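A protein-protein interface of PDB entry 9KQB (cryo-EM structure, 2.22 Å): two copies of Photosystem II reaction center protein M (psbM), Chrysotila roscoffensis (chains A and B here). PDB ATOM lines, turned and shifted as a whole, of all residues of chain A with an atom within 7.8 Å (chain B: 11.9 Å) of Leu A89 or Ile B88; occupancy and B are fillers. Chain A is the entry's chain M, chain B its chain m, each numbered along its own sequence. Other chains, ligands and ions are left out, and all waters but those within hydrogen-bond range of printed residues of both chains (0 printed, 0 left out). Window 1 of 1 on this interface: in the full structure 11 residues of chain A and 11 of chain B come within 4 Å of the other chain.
Of the 15 printed residues of chain A, 5 touch a printed residue of chain B.
Hydrophobic or aromatic side chains of chain A within 4 Å of the printed part of chain B: Phe A81, Phe A84, Leu A85, Ile A88 and Leu A89.
Along chain A the printed residues that touch a printed residue of chain B span positions 81 to 89.
Printed residues of chain B that touch a printed residue of chain A: Phe B81, Phe B84, Leu B85, Ile B88 and Leu B89.
Of the printed residues of chain B, Phe A81 touches Phe B81 and Phe B84.
Printed residues of chain B within 4 Å of Phe A84: Phe B81 (3.4 Å).
Leu A85 touches one residue of chain B.
No residue of chain B comes within 4 Å of Ala A86.
No residue of chain B comes within 4 Å of Val A87.
Of the printed residues of chain B, Ile A88 touches Leu B89 (3.97 Å).
Of chain B, only Ile B88 (3.96 Å) comes within 4 Å of Leu A89.
No residue of chain B comes within 4 Å of Gly A90.
No residue of chain B comes within 4 Å of Leu A91.
Phe A92 touches none of the printed residues of chain B.
Printed residues of chain A within 4 Å of Phe B81: Phe A81 (3.8 Å) and Phe A84 (3.4 Å).
Of the printed residues of chain A, Phe B84 touches Phe A81 (3.4 Å).
Of chain A, only Leu A89 comes within 4 Å of Ile B88.
Of the printed residues of chain A, Leu B89 touches Ile A88 (3.97 Å).
The nearest residue of chain B that does not touch Leu A89 is Leu B89 (4.6 Å).
The nearest residue of chain A that does not touch Ile B88 is Leu A85 (4.4 Å).
Among the printed residues, pairs that only touch across the chains: Phe A81 with Phe B81 (3.8 Å), Phe A81 with Phe B84 (3.4 Å), Phe A84 with Phe B81 (3.4 Å), Leu A85 with Leu B85 (3.8 Å), Ile A88 with Leu B89 (3.97 Å) and Leu A89 with Ile B88 (3.96 Å).
Phe B81 touches its own counterpart, Phe A81.
Phe A81 touches Phe B84, and with the chains exchanged Phe A84 touches Phe B81.
Leu A85 touches its own counterpart, Leu B85.
Ile A88 touches Leu B89, and with the chains exchanged Leu A89 touches Ile B88.
Positions printed for both chains: 81, 82, 83, 84, 85, 86, 87, 88, 89, 90, 91, 92, 93, 94 and 95.
Of the 6 pairs that touch across the chains among the printed residues, 6 have their exchanged pair printed and touching as well.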
ATOM      1  N   PHE A  81      15.375  -6.730  -5.988  1.00  0.00           N
ATOM      2  CA  PHE A  81      16.104  -7.631  -6.875  1.00  0.00           C
ATOM      3  C   PHE A  81      17.383  -8.150  -6.226  1.00  0.00           C
ATOM      4  O   PHE A  81      17.722  -9.331  -6.367  1.00  0.00           O
ATOM      5  CB  PHE A  81      16.403  -6.908  -8.190  1.00  0.00           C
ATOM      6  CG  PHE A  81      17.641  -7.387  -8.888  1.00  0.00           C
ATOM      7  CD1 PHE A  81      17.672  -8.626  -9.506  1.00  0.00           C
ATOM      8  CD2 PHE A  81      18.764  -6.578  -8.957  1.00  0.00           C
ATOM      9  CE1 PHE A  81      18.808  -9.058 -10.146  1.00  0.00           C
ATOM     10  CE2 PHE A  81      19.904  -7.006  -9.604  1.00  0.00           C
ATOM     11  CZ  PHE A  81      19.923  -8.246 -10.203  1.00  0.00           C
ATOM     12  N   GLY A  82      18.109  -7.284  -5.517  1.00  0.00           N
ATOM     13  CA  GLY A  82      19.329  -7.723  -4.860  1.00  0.00           C
ATOM     14  C   GLY A  82      19.065  -8.673  -3.708  1.00  0.00           C
ATOM     15  O   GLY A  82      19.895  -9.527  -3.392  1.00  0.00           O
ATOM     16  N   ALA A  83      17.903  -8.536  -3.065  1.00  0.00           N
ATOM     17  CA  ALA A  83      17.558  -9.408  -1.948  1.00  0.00           C
ATOM     18  C   ALA A  83      17.289 -10.832  -2.411  1.00  0.00           C
ATOM     19  O   ALA A  83      17.557 -11.788  -1.675  1.00  0.00           O
ATOM     20  CB  ALA A  83      16.344  -8.854  -1.212  1.00  0.00           C
ATOM     21  N   PHE A  84      16.735 -10.989  -3.615  1.00  0.00           N
ATOM     22  CA  PHE A  84      16.486 -12.322  -4.157  1.00  0.00           C
ATOM     23  C   PHE A  84      17.791 -13.064  -4.404  1.00  0.00           C
ATOM     24  O   PHE A  84      17.894 -14.267  -4.143  1.00  0.00           O
ATOM     25  CB  PHE A  84      15.682 -12.220  -5.449  1.00  0.00           C
ATOM     26  CG  PHE A  84      14.196 -12.177  -5.245  1.00  0.00           C
ATOM     27  CD1 PHE A  84      13.473 -13.345  -5.071  1.00  0.00           C
ATOM     28  CD2 PHE A  84      13.519 -10.970  -5.246  1.00  0.00           C
ATOM     29  CE1 PHE A  84      12.103 -13.305  -4.890  1.00  0.00           C
ATOM     30  CE2 PHE A  84      12.152 -10.922  -5.064  1.00  0.00           C
ATOM     31  CZ  PHE A  84      11.443 -12.092  -4.886  1.00  0.00           C
ATOM     32  N   LEU A  85      18.799 -12.359  -4.922  1.00  0.00           N
ATOM     33  CA  LEU A  85      20.095 -12.985  -5.154  1.00  0.00           C
ATOM     34  C   LEU A  85      20.792 -13.315  -3.843  1.00  0.00           C
ATOM     35  O   LEU A  85      21.522 -14.307  -3.754  1.00  0.00           O
ATOM     36  CB  LEU A  85      20.978 -12.079  -6.008  1.00  0.00           C
ATOM     37  CG  LEU A  85      20.664 -12.005  -7.499  1.00  0.00           C
ATOM     38  CD1 LEU A  85      21.292 -10.761  -8.088  1.00  0.00           C
ATOM     39  CD2 LEU A  85      21.154 -13.252  -8.213  1.00  0.00           C
ATOM     40  N   ALA A  86      20.590 -12.484  -2.816  1.00  0.00           N
ATOM     41  CA  ALA A  86      21.194 -12.748  -1.514  1.00  0.00           C
ATOM     42  C   ALA A  86      20.642 -14.026  -0.899  1.00  0.00           C
ATOM     43  O   ALA A  86      21.385 -14.806  -0.295  1.00  0.00           O
ATOM     44  CB  ALA A  86      20.967 -11.561  -0.580  1.00  0.00           C
ATOM     45  N   VAL A  87      19.334 -14.252  -1.035  1.00  0.00           N
ATOM     46  CA  VAL A  87      18.731 -15.475  -0.518  1.00  0.00           C
ATOM     47  C   VAL A  87      19.143 -16.674  -1.367  1.00  0.00           C
ATOM     48  O   VAL A  87      19.480 -17.741  -0.840  1.00  0.00           O
ATOM     49  CB  VAL A  87      17.200 -15.325  -0.449  1.00  0.00           C
ATOM     50  CG1 VAL A  87      16.547 -16.628  -0.016  1.00  0.00           C
ATOM     51  CG2 VAL A  87      16.825 -14.201   0.500  1.00  0.00           C
ATOM     52  N   ILE A  88      19.137 -16.511  -2.693  1.00  0.00           N
ATOM     53  CA  ILE A  88      19.418 -17.633  -3.588  1.00  0.00           C
ATOM     54  C   ILE A  88      20.896 -18.009  -3.531  1.00  0.00           C
ATOM     55  O   ILE A  88      21.249 -19.166  -3.282  1.00  0.00           O
ATOM     56  CB  ILE A  88      18.973 -17.302  -5.025  1.00  0.00           C
ATOM     57  CG1 ILE A  88      17.447 -17.379  -5.166  1.00  0.00           C
ATOM     58  CG2 ILE A  88      19.623 -18.248  -6.026  1.00  0.00           C
ATOM     59  CD1 ILE A  88      16.769 -18.447  -4.322  1.00  0.00           C
ATOM     60  N   LEU A  89      21.781 -17.030  -3.744  1.00  0.00           N
ATOM     61  CA  LEU A  89      23.209 -17.336  -3.757  1.00  0.00           C
ATOM     62  C   LEU A  89      23.749 -17.574  -2.354  1.00  0.00           C
ATOM     63  O   LEU A  89      24.708 -18.332  -2.183  1.00  0.00           O
ATOM     64  CB  LEU A  89      23.989 -16.218  -4.448  1.00  0.00           C
ATOM     65  CG  LEU A  89      23.673 -15.964  -5.926  1.00  0.00           C
ATOM     66  CD1 LEU A  89      24.786 -15.160  -6.576  1.00  0.00           C
ATOM     67  CD2 LEU A  89      23.450 -17.269  -6.681  1.00  0.00           C
ATOM     68  N   GLY A  90      23.149 -16.947  -1.343  1.00  0.00           N
ATOM     69  CA  GLY A  90      23.535 -17.230   0.027  1.00  0.00           C
ATOM     70  C   GLY A  90      23.152 -18.613   0.499  1.00  0.00           C
ATOM     71  O   GLY A  90      23.697 -19.080   1.505  1.00  0.00           O
ATOM     72  N   LEU A  91      22.227 -19.269  -0.195  1.00  0.00           N
ATOM     73  CA  LEU A  91      21.859 -20.651   0.066  1.00  0.00           C
ATOM     74  C   LEU A  91      22.533 -21.619  -0.894  1.00  0.00           C
ATOM     75  O   LEU A  91      22.987 -22.681  -0.470  1.00  0.00           O
ATOM     76  CB  LEU A  91      20.332 -20.812  -0.015  1.00  0.00           C
ATOM     77  CG  LEU A  91      19.756 -22.230  -0.048  1.00  0.00           C
ATOM     78  CD1 LEU A  91      19.620 -22.796   1.353  1.00  0.00           C
ATOM     79  CD2 LEU A  91      18.418 -22.246  -0.765  1.00  0.00           C
ATOM     80  N   PHE A  92      22.629 -21.263  -2.178  1.00  0.00           N
ATOM     81  CA  PHE A  92      23.125 -22.197  -3.186  1.00  0.00           C
ATOM     82  C   PHE A  92      24.613 -22.486  -3.013  1.00  0.00           C
ATOM     83  O   PHE A  92      25.029 -23.648  -2.994  1.00  0.00           O
ATOM     84  CB  PHE A  92      22.846 -21.655  -4.589  1.00  0.00           C
ATOM     85  N   ILE A  93      25.427 -21.441  -2.880  1.00  0.00           N
ATOM     86  CA  ILE A  93      26.887 -21.576  -2.836  1.00  0.00           C
ATOM     87  C   ILE A  93      27.375 -22.406  -1.644  1.00  0.00           C
ATOM     88  O   ILE A  93      28.187 -23.317  -1.864  1.00  0.00           O
ATOM     89  CB  ILE A  93      27.571 -20.195  -2.902  1.00  0.00           C
ATOM     90  CG1 ILE A  93      27.534 -19.650  -4.331  1.00  0.00           C
ATOM     91  CG2 ILE A  93      29.011 -20.259  -2.409  1.00  0.00           C
ATOM     92  CD1 ILE A  93      27.147 -18.196  -4.424  1.00  0.00           C
ATOM     93  N   PRO A  94      26.936 -22.187  -0.388  1.00  0.00           N
ATOM     94  CA  PRO A  94      27.419 -23.096   0.671  1.00  0.00           C
ATOM     95  C   PRO A  94      26.835 -24.497   0.583  1.00  0.00           C
ATOM     96  O   PRO A  94      27.499 -25.455   0.997  1.00  0.00           O
ATOM     97  CB  PRO A  94      27.011 -22.388   1.969  1.00  0.00           C
ATOM     98  CG  PRO A  94      25.930 -21.499   1.600  1.00  0.00           C
ATOM     99  CD  PRO A  94      26.167 -21.070   0.200  1.00  0.00           C
ATOM    100  N   VAL A  95      25.612 -24.647   0.063  1.00  0.00           N
ATOM    101  CA  VAL A  95      25.038 -25.978  -0.138  1.00  0.00           C
ATOM    102  C   VAL A  95      25.848 -26.739  -1.181  1.00  0.00           C
ATOM    103  O   VAL A  95      26.134 -27.933  -1.029  1.00  0.00           O
ATOM    104  CB  VAL A  95      23.551 -25.867  -0.530  1.00  0.00           C
ATOM    105  CG1 VAL A  95      23.081 -27.070  -1.339  1.00  0.00           C
ATOM    106  CG2 VAL A  95      22.689 -25.697   0.709  1.00  0.00           C
ATOM    107  N   SER B  80      15.195  -6.606 -16.053  1.00  0.00           N
ATOM    108  CA  SER B  80      14.348  -7.795 -16.016  1.00  0.00           C
ATOM    109  C   SER B  80      14.839  -8.697 -14.893  1.00  0.00           C
ATOM    110  O   SER B  80      15.933  -9.260 -14.965  1.00  0.00           O
ATOM    111  CB  SER B  80      14.369  -8.513 -17.359  1.00  0.00           C
ATOM    112  OG  SER B  80      13.515  -9.644 -17.341  1.00  0.00           O
ATOM    113  N   PHE B  81      14.022  -8.823 -13.844  1.00  0.00           N
ATOM    114  CA  PHE B  81      14.428  -9.561 -12.651  1.00  0.00           C
ATOM    115  C   PHE B  81      14.624 -11.044 -12.937  1.00  0.00           C
ATOM    116  O   PHE B  81      15.603 -11.646 -12.479  1.00  0.00           O
ATOM    117  CB  PHE B  81      13.392  -9.358 -11.545  1.00  0.00           C
ATOM    118  CG  PHE B  81      13.402 -10.436 -10.507  1.00  0.00           C
ATOM    119  CD1 PHE B  81      14.440 -10.526  -9.596  1.00  0.00           C
ATOM    120  CD2 PHE B  81      12.372 -11.361 -10.439  1.00  0.00           C
ATOM    121  CE1 PHE B  81      14.454 -11.519  -8.648  1.00  0.00           C
ATOM    122  CE2 PHE B  81      12.380 -12.358  -9.486  1.00  0.00           C
ATOM    123  CZ  PHE B  81      13.424 -12.436  -8.588  1.00  0.00           C
ATOM    124  N   GLY B  82      13.701 -11.654 -13.682  1.00  0.00           N
ATOM    125  CA  GLY B  82      13.815 -13.077 -13.963  1.00  0.00           C
ATOM    126  C   GLY B  82      14.946 -13.397 -14.921  1.00  0.00           C
ATOM    127  O   GLY B  82      15.477 -14.510 -14.919  1.00  0.00           O
ATOM    128  N   ALA B  83      15.324 -12.427 -15.756  1.00  0.00           N
ATOM    129  CA  ALA B  83      16.425 -12.636 -16.689  1.00  0.00           C
ATOM    130  C   ALA B  83      17.763 -12.745 -15.973  1.00  0.00           C
ATOM    131  O   ALA B  83      18.665 -13.438 -16.455  1.00  0.00           O
ATOM    132  CB  ALA B  83      16.472 -11.503 -17.708  1.00  0.00           C
ATOM    133  N   PHE B  84      17.915 -12.051 -14.844  1.00  0.00           N
ATOM    134  CA  PHE B  84      19.150 -12.138 -14.074  1.00  0.00           C
ATOM    135  C   PHE B  84      19.327 -13.530 -13.484  1.00  0.00           C
ATOM    136  O   PHE B  84      20.437 -14.075 -13.469  1.00  0.00           O
ATOM    137  CB  PHE B  84      19.151 -11.089 -12.967  1.00  0.00           C
ATOM    138  CG  PHE B  84      19.686  -9.754 -13.392  1.00  0.00           C
ATOM    139  CD1 PHE B  84      21.045  -9.492 -13.351  1.00  0.00           C
ATOM    140  CD2 PHE B  84      18.828  -8.756 -13.819  1.00  0.00           C
ATOM    141  CE1 PHE B  84      21.536  -8.259 -13.737  1.00  0.00           C
ATOM    142  CE2 PHE B  84      19.312  -7.523 -14.207  1.00  0.00           C
ATOM    143  CZ  PHE B  84      20.669  -7.275 -14.166  1.00  0.00           C
ATOM    144  N   LEU B  85      18.239 -14.117 -12.980  1.00  0.00           N
ATOM    145  CA  LEU B  85      18.308 -15.474 -12.450  1.00  0.00           C
ATOM    146  C   LEU B  85      18.563 -16.485 -13.559  1.00  0.00           C
ATOM    147  O   LEU B  85      19.231 -17.500 -13.337  1.00  0.00           O
ATOM    148  CB  LEU B  85      17.023 -15.817 -11.697  1.00  0.00           C
ATOM    149  CG  LEU B  85      16.784 -15.159 -10.334  1.00  0.00           C
ATOM    150  CD1 LEU B  85      18.092 -15.045  -9.565  1.00  0.00           C
ATOM    151  CD2 LEU B  85      16.112 -13.802 -10.465  1.00  0.00           C
ATOM    152  N   ALA B  86      18.031 -16.228 -14.756  1.00  0.00           N
ATOM    153  CA  ALA B  86      18.250 -17.131 -15.883  1.00  0.00           C
ATOM    154  C   ALA B  86      19.719 -17.168 -16.282  1.00  0.00           C
ATOM    155  O   ALA B  86      20.260 -18.230 -16.606  1.00  0.00           O
ATOM    156  CB  ALA B  86      17.381 -16.711 -17.068  1.00  0.00           C
ATOM    157  N   VAL B  87      20.377 -16.009 -16.281  1.00  0.00           N
ATOM    158  CA  VAL B  87      21.800 -15.958 -16.602  1.00  0.00           C
ATOM    159  C   VAL B  87      22.625 -16.555 -15.467  1.00  0.00           C
ATOM    160  O   VAL B  87      23.569 -17.319 -15.701  1.00  0.00           O
ATOM    161  CB  VAL B  87      22.224 -14.511 -16.918  1.00  0.00           C
ATOM    162  CG1 VAL B  87      23.724 -14.423 -17.143  1.00  0.00           C
ATOM    163  CG2 VAL B  87      21.475 -13.999 -18.135  1.00  0.00           C
ATOM    164  N   ILE B  88      22.271 -16.230 -14.221  1.00  0.00           N
ATOM    165  CA  ILE B  88      23.069 -16.667 -13.076  1.00  0.00           C
ATOM    166  C   ILE B  88      22.891 -18.163 -12.838  1.00  0.00           C
ATOM    167  O   ILE B  88      23.866 -18.922 -12.805  1.00  0.00           O
ATOM    168  CB  ILE B  88      22.710 -15.846 -11.822  1.00  0.00           C
ATOM    169  CG1 ILE B  88      23.305 -14.434 -11.892  1.00  0.00           C
ATOM    170  CG2 ILE B  88      23.207 -16.538 -10.561  1.00  0.00           C
ATOM    171  CD1 ILE B  88      24.654 -14.330 -12.585  1.00  0.00           C
ATOM    172  N   LEU B  89      21.643 -18.611 -12.678  1.00  0.00           N
ATOM    173  CA  LEU B  89      21.406 -20.022 -12.386  1.00  0.00           C
ATOM    174  C   LEU B  89      21.638 -20.890 -13.614  1.00  0.00           C
ATOM    175  O   LEU B  89      21.990 -22.069 -13.491  1.00  0.00           O
ATOM    176  CB  LEU B  89      19.992 -20.225 -11.842  1.00  0.00           C
ATOM    177  CG  LEU B  89      19.665 -19.562 -10.501  1.00  0.00           C
ATOM    178  CD1 LEU B  89      18.413 -20.175  -9.896  1.00  0.00           C
ATOM    179  CD2 LEU B  89      20.834 -19.668  -9.530  1.00  0.00           C
ATOM    180  N   GLY B  90      21.449 -20.328 -14.809  1.00  0.00           N
ATOM    181  CA  GLY B  90      21.763 -21.057 -16.022  1.00  0.00           C
ATOM    182  C   GLY B  90      23.245 -21.277 -16.218  1.00  0.00           C
ATOM    183  O   GLY B  90      23.638 -22.185 -16.957  1.00  0.00           O
ATOM    184  N   LEU B  91      24.079 -20.459 -15.581  1.00  0.00           N
ATOM    185  CA  LEU B  91      25.523 -20.632 -15.595  1.00  0.00           C
ATOM    186  C   LEU B  91      26.026 -21.377 -14.366  1.00  0.00           C
ATOM    187  O   LEU B  91      26.885 -22.252 -14.489  1.00  0.00           O
ATOM    188  CB  LEU B  91      26.217 -19.266 -15.697  1.00  0.00           C
ATOM    189  CG  LEU B  91      27.721 -19.209 -15.424  1.00  0.00           C
ATOM    190  CD1 LEU B  91      28.515 -19.629 -16.647  1.00  0.00           C
ATOM    191  CD2 LEU B  91      28.131 -17.819 -14.969  1.00  0.00           C
ATOM    192  N   PHE B  92      25.486 -21.067 -13.185  1.00  0.00           N
ATOM    193  CA  PHE B  92      26.027 -21.608 -11.940  1.00  0.00           C
ATOM    194  C   PHE B  92      25.773 -23.106 -11.813  1.00  0.00           C
ATOM    195  O   PHE B  92      26.691 -23.875 -11.510  1.00  0.00           O
ATOM    196  CB  PHE B  92      25.437 -20.862 -10.743  1.00  0.00           C
ATOM    197  N   ILE B  93      24.535 -23.537 -12.044  1.00  0.00           N
ATOM    198  CA  ILE B  93      24.131 -24.929 -11.823  1.00  0.00           C
ATOM    199  C   ILE B  93      24.884 -25.921 -12.716  1.00  0.00           C
ATOM    200  O   ILE B  93      25.394 -26.915 -12.178  1.00  0.00           O
ATOM    201  CB  ILE B  93      22.600 -25.081 -11.947  1.00  0.00           C
ATOM    202  CG1 ILE B  93      21.914 -24.592 -10.672  1.00  0.00           C
ATOM    203  CG2 ILE B  93      22.204 -26.521 -12.217  1.00  0.00           C
ATOM    204  CD1 ILE B  93      20.679 -23.765 -10.918  1.00  0.00           C
ATOM    205  N   PRO B  94      25.023 -25.733 -14.044  1.00  0.00           N
ATOM    206  CA  PRO B  94      25.835 -26.713 -14.792  1.00  0.00           C
ATOM    207  C   PRO B  94      27.324 -26.617 -14.502  1.00  0.00           C
ATOM    208  O   PRO B  94      28.022 -27.633 -14.586  1.00  0.00           O
ATOM    209  CB  PRO B  94      25.518 -26.399 -16.260  1.00  0.00           C
ATOM    210  CG  PRO B  94      25.056 -25.032 -16.267  1.00  0.00           C
ATOM    211  CD  PRO B  94      24.368 -24.788 -14.974  1.00  0.00           C
ATOM    212  N   VAL B  95      27.831 -25.427 -14.168  1.00  0.00           N
ATOM    213  CA  VAL B  95      29.232 -25.295 -13.766  1.00  0.00           C
ATOM    214  C   VAL B  95      29.476 -26.050 -12.466  1.00  0.00           C
ATOM    215  O   VAL B  95      30.496 -26.734 -12.305  1.00  0.00           O
ATOM    216  CB  VAL B  95      29.615 -23.803 -13.654  1.00  0.00           C
ATOM    217  CG1 VAL B  95      30.792 -23.587 -12.709  1.00  0.00           C
ATOM    218  CG2 VAL B  95      29.935 -23.235 -15.025  1.00  0.00           C
ATOM    219  N   VAL B  96      28.525 -25.961 -11.535  1.00  0.00           N
ATOM    220  CA  VAL B  96      28.612 -26.686 -10.269  1.00  0.00           C
ATOM    221  C   VAL B  96      28.610 -28.191 -10.516  1.00  0.00           C
ATOM    222  O   VAL B  96      29.397 -28.938  -9.922  1.00  0.00           O
ATOM    223  CB  VAL B  96      27.458 -26.259  -9.345  1.00  0.00           C
ATOM    224  CG1 VAL B  96      27.105 -27.356  -8.351  1.00  0.00           C
ATOM    225  CG2 VAL B  96      27.799 -24.953  -8.647  1.00  0.00           C
ATOM    226  N   PHE B  97      27.732 -28.648 -11.413  1.00  0.00           N
ATOM    227  CA  PHE B  97      27.628 -30.072 -11.722  1.00  0.00           C
ATOM    228  C   PHE B  97      28.912 -30.602 -12.351  1.00  0.00           C
ATOM    229  O   PHE B  97      29.338 -31.725 -12.055  1.00  0.00           O
ATOM    230  CB  PHE B  97      26.422 -30.302 -12.637  1.00  0.00           C
ATOM    231  CG  PHE B  97      26.554 -31.489 -13.550  1.00  0.00           C
ATOM    232  CD1 PHE B  97      26.367 -32.774 -13.070  1.00  0.00           C
ATOM    233  CD2 PHE B  97      26.834 -31.316 -14.897  1.00  0.00           C
ATOM    234  CE1 PHE B  97      26.477 -33.864 -13.908  1.00  0.00           C
ATOM    235  CE2 PHE B  97      26.948 -32.403 -15.740  1.00  0.00           C
ATOM    236  CZ  PHE B  97      26.768 -33.679 -15.244  1.00  0.00           C
